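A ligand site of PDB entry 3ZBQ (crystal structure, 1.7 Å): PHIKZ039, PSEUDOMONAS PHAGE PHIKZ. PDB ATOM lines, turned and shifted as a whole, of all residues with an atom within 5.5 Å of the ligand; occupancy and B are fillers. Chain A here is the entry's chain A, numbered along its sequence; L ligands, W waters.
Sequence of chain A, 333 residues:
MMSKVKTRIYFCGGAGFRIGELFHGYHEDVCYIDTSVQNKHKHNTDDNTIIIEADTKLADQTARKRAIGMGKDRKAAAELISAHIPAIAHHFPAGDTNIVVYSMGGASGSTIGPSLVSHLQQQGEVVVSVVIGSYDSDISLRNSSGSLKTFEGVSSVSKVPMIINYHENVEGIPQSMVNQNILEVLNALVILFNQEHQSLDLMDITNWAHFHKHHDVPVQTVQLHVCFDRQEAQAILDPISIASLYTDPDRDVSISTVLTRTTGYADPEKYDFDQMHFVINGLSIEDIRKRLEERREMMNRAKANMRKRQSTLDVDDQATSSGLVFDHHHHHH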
ATOM      1  N   CYS A  12     -32.783  27.039 -28.002  1.00  0.00           N
ATOM      2  CA  CYS A  12     -32.491  27.644 -26.712  1.00  0.00           C
ATOM      3  C   CYS A  12     -30.997  27.774 -26.448  1.00  0.00           C
ATOM      4  O   CYS A  12     -30.226  26.831 -26.647  1.00  0.00           O
ATOM      5  CB  CYS A  12     -33.132  26.827 -25.568  1.00  0.00           C
ATOM      6  SG  CYS A  12     -34.867  26.431 -25.802  1.00  0.00           S
ATOM      7  N   GLY A  13     -30.608  28.955 -25.971  1.00  0.00           N
ATOM      8  CA  GLY A  13     -29.220  29.230 -25.651  1.00  0.00           C
ATOM      9  C   GLY A  13     -28.364  29.352 -26.907  1.00  0.00           C
ATOM     10  O   GLY A  13     -28.888  29.262 -28.008  1.00  0.00           O
ATOM     11  N   GLY A  14     -27.058  29.536 -26.733  1.00  0.00           N
ATOM     12  CA  GLY A  14     -26.155  29.749 -27.857  1.00  0.00           C
ATOM     13  C   GLY A  14     -26.160  28.637 -28.893  1.00  0.00           C
ATOM     14  O   GLY A  14     -26.334  28.891 -30.079  1.00  0.00           O
ATOM     15  N   ALA A  15     -25.967  27.405 -28.444  1.00  0.00           N
ATOM     16  CA  ALA A  15     -25.897  26.277 -29.360  1.00  0.00           C
ATOM     17  C   ALA A  15     -27.214  26.191 -30.135  1.00  0.00           C
ATOM     18  O   ALA A  15     -27.203  25.910 -31.323  1.00  0.00           O
ATOM     19  CB  ALA A  15     -25.629  24.975 -28.621  1.00  0.00           C
ATOM     20  N   GLY A  16     -28.319  26.445 -29.450  1.00  0.00           N
ATOM     21  CA  GLY A  16     -29.633  26.398 -30.078  1.00  0.00           C
ATOM     22  C   GLY A  16     -29.757  27.465 -31.140  1.00  0.00           C
ATOM     23  O   GLY A  16     -30.232  27.205 -32.238  1.00  0.00           O
ATOM     24  N   ARG A  18     -27.277  28.877 -32.832  1.00  0.00           N
ATOM     25  CA  ARG A  18     -26.379  28.572 -33.940  1.00  0.00           C
ATOM     26  C   ARG A  18     -26.925  27.471 -34.830  1.00  0.00           C
ATOM     27  O   ARG A  18     -26.872  27.565 -36.064  1.00  0.00           O
ATOM     28  CB  ARG A  18     -24.984  28.204 -33.408  1.00  0.00           C
ATOM     29  CG  ARG A  18     -24.191  29.427 -32.926  1.00  0.00           C
ATOM     30  CD  ARG A  18     -23.285  29.113 -31.741  1.00  0.00           C
ATOM     31  NE  ARG A  18     -23.175  30.249 -30.808  1.00  0.00           N
ATOM     32  CZ  ARG A  18     -22.991  30.131 -29.498  1.00  0.00           C
ATOM     33  NH1 ARG A  18     -22.855  28.919 -28.956  1.00  0.00           N
ATOM     34  NH2 ARG A  18     -22.916  31.211 -28.729  1.00  0.00           N
ATOM     35  N   ILE A  19     -27.470  26.433 -34.215  1.00  0.00           N
ATOM     36  CA  ILE A  19     -28.110  25.363 -34.977  1.00  0.00           C
ATOM     37  C   ILE A  19     -29.309  25.927 -35.747  1.00  0.00           C
ATOM     38  O   ILE A  19     -29.517  25.607 -36.931  1.00  0.00           O
ATOM     39  CB  ILE A  19     -28.592  24.232 -34.057  1.00  0.00           C
ATOM     40  CG1 ILE A  19     -27.392  23.505 -33.418  1.00  0.00           C
ATOM     41  CG2 ILE A  19     -29.482  23.263 -34.831  1.00  0.00           C
ATOM     42  CD1 ILE A  19     -26.442  22.885 -34.432  1.00  0.00           C
ATOM     43  N   ASP A  34     -33.242  32.932 -25.256  1.00  0.00           N
ATOM     44  CA  ASP A  34     -31.899  33.017 -24.702  1.00  0.00           C
ATOM     45  C   ASP A  34     -31.847  34.076 -23.607  1.00  0.00           C
ATOM     46  O   ASP A  34     -32.846  34.750 -23.340  1.00  0.00           O
ATOM     47  CB  ASP A  34     -30.892  33.371 -25.804  1.00  0.00           C
ATOM     48  CG  ASP A  34     -29.470  32.943 -25.479  1.00  0.00           C
ATOM     49  OD1 ASP A  34     -29.180  32.595 -24.310  1.00  0.00           O
ATOM     50  OD2 ASP A  34     -28.640  32.955 -26.415  1.00  0.00           O
ATOM     51  N   ASN A  39     -26.029  36.514 -29.118  1.00  0.00           N
ATOM     52  CA  ASN A  39     -26.218  35.303 -29.907  1.00  0.00           C
ATOM     53  C   ASN A  39     -27.203  35.481 -31.056  1.00  0.00           C
ATOM     54  O   ASN A  39     -27.320  34.609 -31.919  1.00  0.00           O
ATOM     55  CB  ASN A  39     -26.675  34.142 -29.022  1.00  0.00           C
ATOM     56  CG  ASN A  39     -25.551  33.594 -28.170  1.00  0.00           C
ATOM     57  OD1 ASN A  39     -24.375  33.615 -28.567  1.00  0.00           O
ATOM     58  ND2 ASN A  39     -25.894  33.078 -26.998  1.00  0.00           N
ATOM     59  N   MET A  70     -25.141  33.895 -19.403  1.00  0.00           N
ATOM     60  CA  MET A  70     -24.980  33.382 -18.051  1.00  0.00           C
ATOM     61  C   MET A  70     -23.597  32.757 -17.821  1.00  0.00           C
ATOM     62  O   MET A  70     -23.302  32.279 -16.727  1.00  0.00           O
ATOM     63  CB  MET A  70     -26.111  32.398 -17.732  1.00  0.00           C
ATOM     64  CG  MET A  70     -27.450  33.076 -17.520  1.00  0.00           C
ATOM     65  SD  MET A  70     -27.570  33.914 -15.930  1.00  0.00           S
ATOM     66  CE  MET A  70     -27.924  35.573 -16.471  1.00  0.00           C
ATOM     67  N   LYS A  72     -21.990  29.915 -18.486  1.00  0.00           N
ATOM     68  CA  LYS A  72     -21.933  28.552 -17.943  1.00  0.00           C
ATOM     69  C   LYS A  72     -22.327  28.399 -16.469  1.00  0.00           C
ATOM     70  O   LYS A  72     -22.066  27.362 -15.862  1.00  0.00           O
ATOM     71  CB  LYS A  72     -20.575  27.895 -18.243  1.00  0.00           C
ATOM     72  CG  LYS A  72     -20.294  27.779 -19.718  1.00  0.00           C
ATOM     73  CD  LYS A  72     -19.029  26.978 -19.964  1.00  0.00           C
ATOM     74  CE  LYS A  72     -18.751  26.823 -21.451  1.00  0.00           C
ATOM     75  NZ  LYS A  72     -18.436  28.120 -22.117  1.00  0.00           N
ATOM     76  N   SER A 103     -27.542  22.935 -25.812  1.00  0.00           N
ATOM     77  CA  SER A 103     -26.377  22.225 -25.315  1.00  0.00           C
ATOM     78  C   SER A 103     -26.602  21.805 -23.864  1.00  0.00           C
ATOM     79  O   SER A 103     -27.405  22.403 -23.153  1.00  0.00           O
ATOM     80  CB  SER A 103     -25.151  23.133 -25.379  1.00  0.00           C
ATOM     81  OG  SER A 103     -25.352  24.272 -24.571  1.00  0.00           O
ATOM     82  N   GLY A 105     -23.780  21.486 -21.795  1.00  0.00           N
ATOM     83  CA  GLY A 105     -22.640  21.991 -21.029  1.00  0.00           C
ATOM     84  C   GLY A 105     -22.664  23.477 -20.754  1.00  0.00           C
ATOM     85  O   GLY A 105     -21.800  24.006 -20.041  1.00  0.00           O
ATOM     86  N   GLY A 106     -23.647  24.165 -21.339  1.00  0.00           N
ATOM     87  CA  GLY A 106     -23.833  25.577 -21.119  1.00  0.00           C
ATOM     88  C   GLY A 106     -24.768  25.851 -19.960  1.00  0.00           C
ATOM     89  O   GLY A 106     -25.049  24.963 -19.158  1.00  0.00           O
ATOM     90  N   ALA A 107     -25.261  27.086 -19.867  1.00  0.00           N
ATOM     91  CA  ALA A 107     -26.094  27.519 -18.747  1.00  0.00           C
ATOM     92  C   ALA A 107     -27.549  27.791 -19.138  1.00  0.00           C
ATOM     93  O   ALA A 107     -28.466  27.447 -18.399  1.00  0.00           O
ATOM     94  CB  ALA A 107     -25.502  28.764 -18.097  1.00  0.00           C
ATOM     95  N   SER A 108     -27.743  28.418 -20.283  1.00  0.00           N
ATOM     96  CA  SER A 108     -29.061  28.911 -20.661  1.00  0.00           C
ATOM     97  C   SER A 108     -29.858  27.860 -21.421  1.00  0.00           C
ATOM     98  O   SER A 108     -31.015  27.605 -21.084  1.00  0.00           O
ATOM     99  CB  SER A 108     -28.940  30.188 -21.485  1.00  0.00           C
ATOM    100  OG  SER A 108     -28.343  31.206 -20.708  1.00  0.00           O
ATOM    101  N   GLY A 109     -29.234  27.235 -22.409  1.00  0.00           N
ATOM    102  CA  GLY A 109     -29.941  26.196 -23.143  1.00  0.00           C
ATOM    103  C   GLY A 109     -30.276  25.030 -22.239  1.00  0.00           C
ATOM    104  O   GLY A 109     -31.340  24.422 -22.351  1.00  0.00           O
ATOM    105  N   SER A 110     -29.353  24.704 -21.332  1.00  0.00           N
ATOM    106  CA  SER A 110     -29.507  23.526 -20.469  1.00  0.00           C
ATOM    107  C   SER A 110     -30.452  23.749 -19.281  1.00  0.00           C
ATOM    108  O   SER A 110     -30.651  22.856 -18.467  1.00  0.00           O
ATOM    109  CB  SER A 110     -28.165  23.064 -19.951  1.00  0.00           C
ATOM    110  OG  SER A 110     -27.679  23.977 -18.962  1.00  0.00           O
ATOM    111  N   ILE A 132     -26.575  18.463 -26.921  1.00  0.00           N
ATOM    112  CA  ILE A 132     -25.130  18.330 -27.147  1.00  0.00           C
ATOM    113  C   ILE A 132     -24.372  18.197 -25.820  1.00  0.00           C
ATOM    114  O   ILE A 132     -24.400  19.104 -24.979  1.00  0.00           O
ATOM    115  CB  ILE A 132     -24.556  19.552 -27.912  1.00  0.00           C
ATOM    116  CG1 ILE A 132     -25.314  19.760 -29.231  1.00  0.00           C
ATOM    117  CG2 ILE A 132     -23.057  19.378 -28.186  1.00  0.00           C
ATOM    118  CD1 ILE A 132     -25.098  21.127 -29.870  1.00  0.00           C
ATOM    119  N   SER A 134     -20.904  18.043 -23.580  1.00  0.00           N
ATOM    120  CA  SER A 134     -19.526  18.562 -23.667  1.00  0.00           C
ATOM    121  C   SER A 134     -18.844  18.471 -22.311  1.00  0.00           C
ATOM    122  O   SER A 134     -19.494  18.330 -21.273  1.00  0.00           O
ATOM    123  CB  SER A 134     -19.489  19.985 -24.230  1.00  0.00           C
ATOM    124  OG  SER A 134     -20.102  20.927 -23.355  1.00  0.00           O
ATOM    125  N   ASP A 136     -15.302  20.134 -21.914  1.00  0.00           N
ATOM    126  CA  ASP A 136     -14.002  20.790 -22.161  1.00  0.00           C
ATOM    127  C   ASP A 136     -13.416  21.472 -20.940  1.00  0.00           C
ATOM    128  O   ASP A 136     -12.296  21.980 -20.984  1.00  0.00           O
ATOM    129  CB  ASP A 136     -14.075  21.769 -23.360  1.00  0.00           C
ATOM    130  CG  ASP A 136     -14.918  23.010 -23.076  1.00  0.00           C
ATOM    131  OD1 ASP A 136     -15.795  22.954 -22.200  1.00  0.00           O
ATOM    132  OD2 ASP A 136     -14.697  24.048 -23.746  1.00  0.00           O
ATOM    133  N   SER A 140     -18.097  22.841 -17.481  1.00  0.00           N
ATOM    134  CA  SER A 140     -18.976  22.339 -18.539  1.00  0.00           C
ATOM    135  C   SER A 140     -19.292  20.858 -18.347  1.00  0.00           C
ATOM    136  O   SER A 140     -20.394  20.395 -18.698  1.00  0.00           O
ATOM    137  CB  SER A 140     -18.378  22.599 -19.924  1.00  0.00           C
ATOM    138  OG  SER A 140     -17.202  21.847 -20.126  1.00  0.00           O
ATOM    139  N   ASN A 169     -19.973  16.484 -28.241  1.00  0.00           N
ATOM    140  CA  ASN A 169     -18.834  17.240 -28.738  1.00  0.00           C
ATOM    141  C   ASN A 169     -17.591  16.487 -28.308  1.00  0.00           C
ATOM    142  O   ASN A 169     -17.014  16.778 -27.251  1.00  0.00           O
ATOM    143  CB  ASN A 169     -18.809  18.671 -28.171  1.00  0.00           C
ATOM    144  CG  ASN A 169     -19.658  19.650 -28.976  1.00  0.00           C
ATOM    145  OD1 ASN A 169     -20.156  19.330 -30.066  1.00  0.00           O
ATOM    146  ND2 ASN A 169     -19.806  20.870 -28.457  1.00  0.00           N
ATOM    147  N   GLN A 175     -16.792  21.044 -34.264  1.00  0.00           N
ATOM    148  CA  GLN A 175     -18.209  21.131 -33.942  1.00  0.00           C
ATOM    149  C   GLN A 175     -19.064  21.184 -35.204  1.00  0.00           C
ATOM    150  O   GLN A 175     -20.232  20.789 -35.180  1.00  0.00           O
ATOM    151  CB  GLN A 175     -18.484  22.321 -33.027  1.00  0.00           C
ATOM    152  CG  GLN A 175     -17.912  22.142 -31.626  1.00  0.00           C
ATOM    153  CD  GLN A 175     -18.130  23.352 -30.755  1.00  0.00           C
ATOM    154  OE1 GLN A 175     -18.852  24.288 -31.118  1.00  0.00           O
ATOM    155  NE2 GLN A 175     -17.496  23.361 -29.586  1.00  0.00           N
ATOM    156  N   VAL A 178     -20.623  17.841 -35.819  1.00  0.00           N
ATOM    157  CA  VAL A 178     -21.748  17.630 -34.925  1.00  0.00           C
ATOM    158  C   VAL A 178     -22.952  18.428 -35.410  1.00  0.00           C
ATOM    159  O   VAL A 178     -24.071  17.921 -35.433  1.00  0.00           O
ATOM    160  CB  VAL A 178     -21.392  17.978 -33.462  1.00  0.00           C
ATOM    161  CG1 VAL A 178     -22.614  17.861 -32.564  1.00  0.00           C
ATOM    162  CG2 VAL A 178     -20.280  17.076 -32.979  1.00  0.00           C
ATOM    163  N   ASN A 179     -22.728  19.666 -35.839  1.00  0.00           N
ATOM    164  CA  ASN A 179     -23.833  20.497 -36.327  1.00  0.00           C
ATOM    165  C   ASN A 179     -24.507  19.878 -37.536  1.00  0.00           C
ATOM    166  O   ASN A 179     -25.735  19.885 -37.662  1.00  0.00           O
ATOM    167  CB  ASN A 179     -23.349  21.903 -36.664  1.00  0.00           C
ATOM    168  CG  ASN A 179     -22.849  22.644 -35.455  1.00  0.00           C
ATOM    169  OD1 ASN A 179     -23.072  22.205 -34.331  1.00  0.00           O
ATOM    170  ND2 ASN A 179     -22.172  23.763 -35.666  1.00  0.00           N
ATOM    171  N   ILE A 182     -26.682  17.064 -36.525  1.00  0.00           N
ATOM    172  CA  ILE A 182     -27.882  17.611 -35.918  1.00  0.00           C
ATOM    173  C   ILE A 182     -28.887  18.111 -36.952  1.00  0.00           C
ATOM    174  O   ILE A 182     -30.083  17.880 -36.831  1.00  0.00           O
ATOM    175  CB  ILE A 182     -27.533  18.712 -34.889  1.00  0.00           C
ATOM    176  CG1 ILE A 182     -26.933  18.055 -33.626  1.00  0.00           C
ATOM    177  CG2 ILE A 182     -28.762  19.542 -34.560  1.00  0.00           C
ATOM    178  CD1 ILE A 182     -26.372  19.044 -32.609  1.00  0.00           C
HETATM  179  P1  LIG L   1     -25.599  28.573 -23.372  1.00  0.00           P
HETATM  180  O1  LIG L   1     -25.840  29.799 -24.218  1.00  0.00           O
HETATM  181  O2  LIG L   1     -26.728  27.577 -23.557  1.00  0.00           O
HETATM  182  O3  LIG L   1     -25.447  28.915 -21.906  1.00  0.00           O
HETATM  183  O4  LIG L   1     -24.239  27.828 -23.794  1.00  0.00           O
HETATM  184  P2  LIG L   1     -23.749  27.532 -25.296  1.00  0.00           P
HETATM  185  O5  LIG L   1     -23.501  28.750 -26.169  1.00  0.00           O
HETATM  186  O6  LIG L   1     -24.696  26.562 -25.967  1.00  0.00           O
HETATM  187  O7  LIG L   1     -22.349  26.821 -25.030  1.00  0.00           O
HETATM  188  C1  LIG L   1     -22.243  25.673 -24.190  1.00  0.00           C
HETATM  189  C2  LIG L   1     -21.432  24.601 -24.906  1.00  0.00           C
HETATM  190  O8  LIG L   1     -22.172  24.109 -26.020  1.00  0.00           O
HETATM  191  C3  LIG L   1     -20.130  25.105 -25.504  1.00  0.00           C
HETATM  192  O9  LIG L   1     -19.074  25.037 -24.520  1.00  0.00           O
HETATM  193  C4  LIG L   1     -19.898  24.161 -26.652  1.00  0.00           C
HETATM  194  O10 LIG L   1     -19.315  22.953 -26.161  1.00  0.00           O
HETATM  195  C5  LIG L   1     -21.291  23.772 -27.088  1.00  0.00           C
HETATM  196  N1  LIG L   1     -21.748  24.528 -28.268  1.00  0.00           N
HETATM  197  C6  LIG L   1     -22.097  25.823 -28.343  1.00  0.00           C
HETATM  198  N2  LIG L   1     -22.479  26.156 -29.592  1.00  0.00           N
HETATM  199  C7  LIG L   1     -22.388  25.046 -30.364  1.00  0.00           C
HETATM  200  C8  LIG L   1     -22.636  24.674 -31.772  1.00  0.00           C
HETATM  201  O11 LIG L   1     -23.056  25.519 -32.598  1.00  0.00           O
HETATM  202  N3  LIG L   1     -22.403  23.401 -32.121  1.00  0.00           N
HETATM  203  C9  LIG L   1     -21.953  22.472 -31.263  1.00  0.00           C
HETATM  204  N4  LIG L   1     -21.733  21.196 -31.675  1.00  0.00           N
HETATM  205  N5  LIG L   1     -21.705  22.733 -29.956  1.00  0.00           N
HETATM  206  C10 LIG L   1     -21.903  23.980 -29.474  1.00  0.00           C
HETATM  207  O   HOH W   1     -21.723  27.158 -34.204  1.00  0.00           O
HETATM  208  O   HOH W   2     -26.698  25.145 -22.217  1.00  0.00           O
HETATM  209  O   HOH W   3     -18.580  23.109 -23.041  1.00  0.00           O
HETATM  210  O   HOH W   4     -23.655  31.488 -25.481  1.00  0.00           O
HETATM  211  O   HOH W   5     -23.053  29.945 -21.045  1.00  0.00           O
HETATM  212  O   HOH W   6     -26.499  32.387 -23.703  1.00  0.00           O
HETATM  213  O   HOH W   7     -22.661  21.230 -24.376  1.00  0.00           O
HETATM  214  O   HOH W   8     -17.454  27.415 -24.803  1.00  0.00           O
HETATM  215  O   HOH W   9     -25.849  31.819 -21.135  1.00  0.00           O
HETATM  216  O   HOH W  10     -16.589  23.332 -26.037  1.00  0.00           O
HETATM  217  O   HOH W  11     -16.877  20.862 -26.584  1.00  0.00           O
HETATM  218  O   HOH W  12     -27.693  25.891 -25.805  1.00  0.00           O
HETATM  219  O   HOH W  13     -19.959  25.276 -33.689  1.00  0.00           O
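The backbone NH (N) of Ser 108 is in hydrogen-bond range of an oxygen (O3) of the ligand (2.9 Å). The guanidinium group (NH1) of Arg 18 is in salt-bridge range of an oxygen (O5) of the ligand (2.9 Å). A nitrogen (N3) of the ligand is in hydrogen-bond range of the side-chain amide oxygen (OD1) of Asn 179 (2.6 Å). A nitrogen (N5) of the ligand lies close to the side-chain amide oxygen (OE1) of Gln 175, at 3.5 Å. An oxygen (O6) of the ligand is in hydrogen-bond range of the side-chain hydroxyl (OG) of Ser 103 (2.8 Å). O2 of the ligand is in hydrogen-bond range of N of Gly 109. The backbone NH (N) of Gly 14 lies within hydrogen-bond range of an oxygen (O1) of the ligand (2.8 Å). An oxygen (O3) of the ligand sits at hydrogen-bond distance from the backbone NH (N) of Ala 107 (2.7 Å). OD1 of Asn 169 is in hydrogen-bond range of N4 of the ligand (2.9 Å). An oxygen (O6) of the ligand sits at hydrogen-bond distance from the backbone NH (N) of Ala 15 (2.9 Å).
The guanidinium group (NH2) of Arg 18 sits at hydrogen-bond distance from the side-chain amide oxygen (OD1) of Asn 39 (2.8 Å). OD1 of Asn 179 lies close to O of Gln 175, 3.3 Å away. The backbone carbonyl oxygen (O) of Gly 106 is in hydrogen-bond range of the side-chain hydroxyl (OG) of Ser 110, 2.8 Å away.
Merely in contact with the ligand: Gly 106 (3.5 Å), Ser 134 (3.5 Å), Val 178 (3.6 Å), Lys 72 (3.6 Å), Gly 13 (3.7 Å) and Ile 132 (3.7 Å).
Water W6 lies within hydrogen-bond range of an oxygen (O1) of the ligand, the side-chain carboxylate of Asp 34 and the side-chain amide nitrogen of Asn 39. Water W5 lies within hydrogen-bond range of an oxygen (O3) of the ligand and the backbone NH of Lys 72. Water W8 bridges O9 of the ligand (2.9 Å) and NZ of Lys 72 (2.9 Å). Water W12 lies within hydrogen-bond range of O of Cys 12 (2.8 Å), N of Ser 103 (3.0 Å), O2 of the ligand (3.0 Å) and N of Ala 15 (3.5 Å). Water W13 lies within hydrogen-bond range of OE1 of Gln 175 (3.0 Å), O11 of the ligand (3.3 Å) and ND2 of Asn 179 (3.3 Å). Water W7 lies within hydrogen-bond range of the side-chain hydroxyl of Ser 134, the backbone carbonyl oxygen of Ile 132, the backbone NH of Gly 105 and an oxygen (O8) of the ligand.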
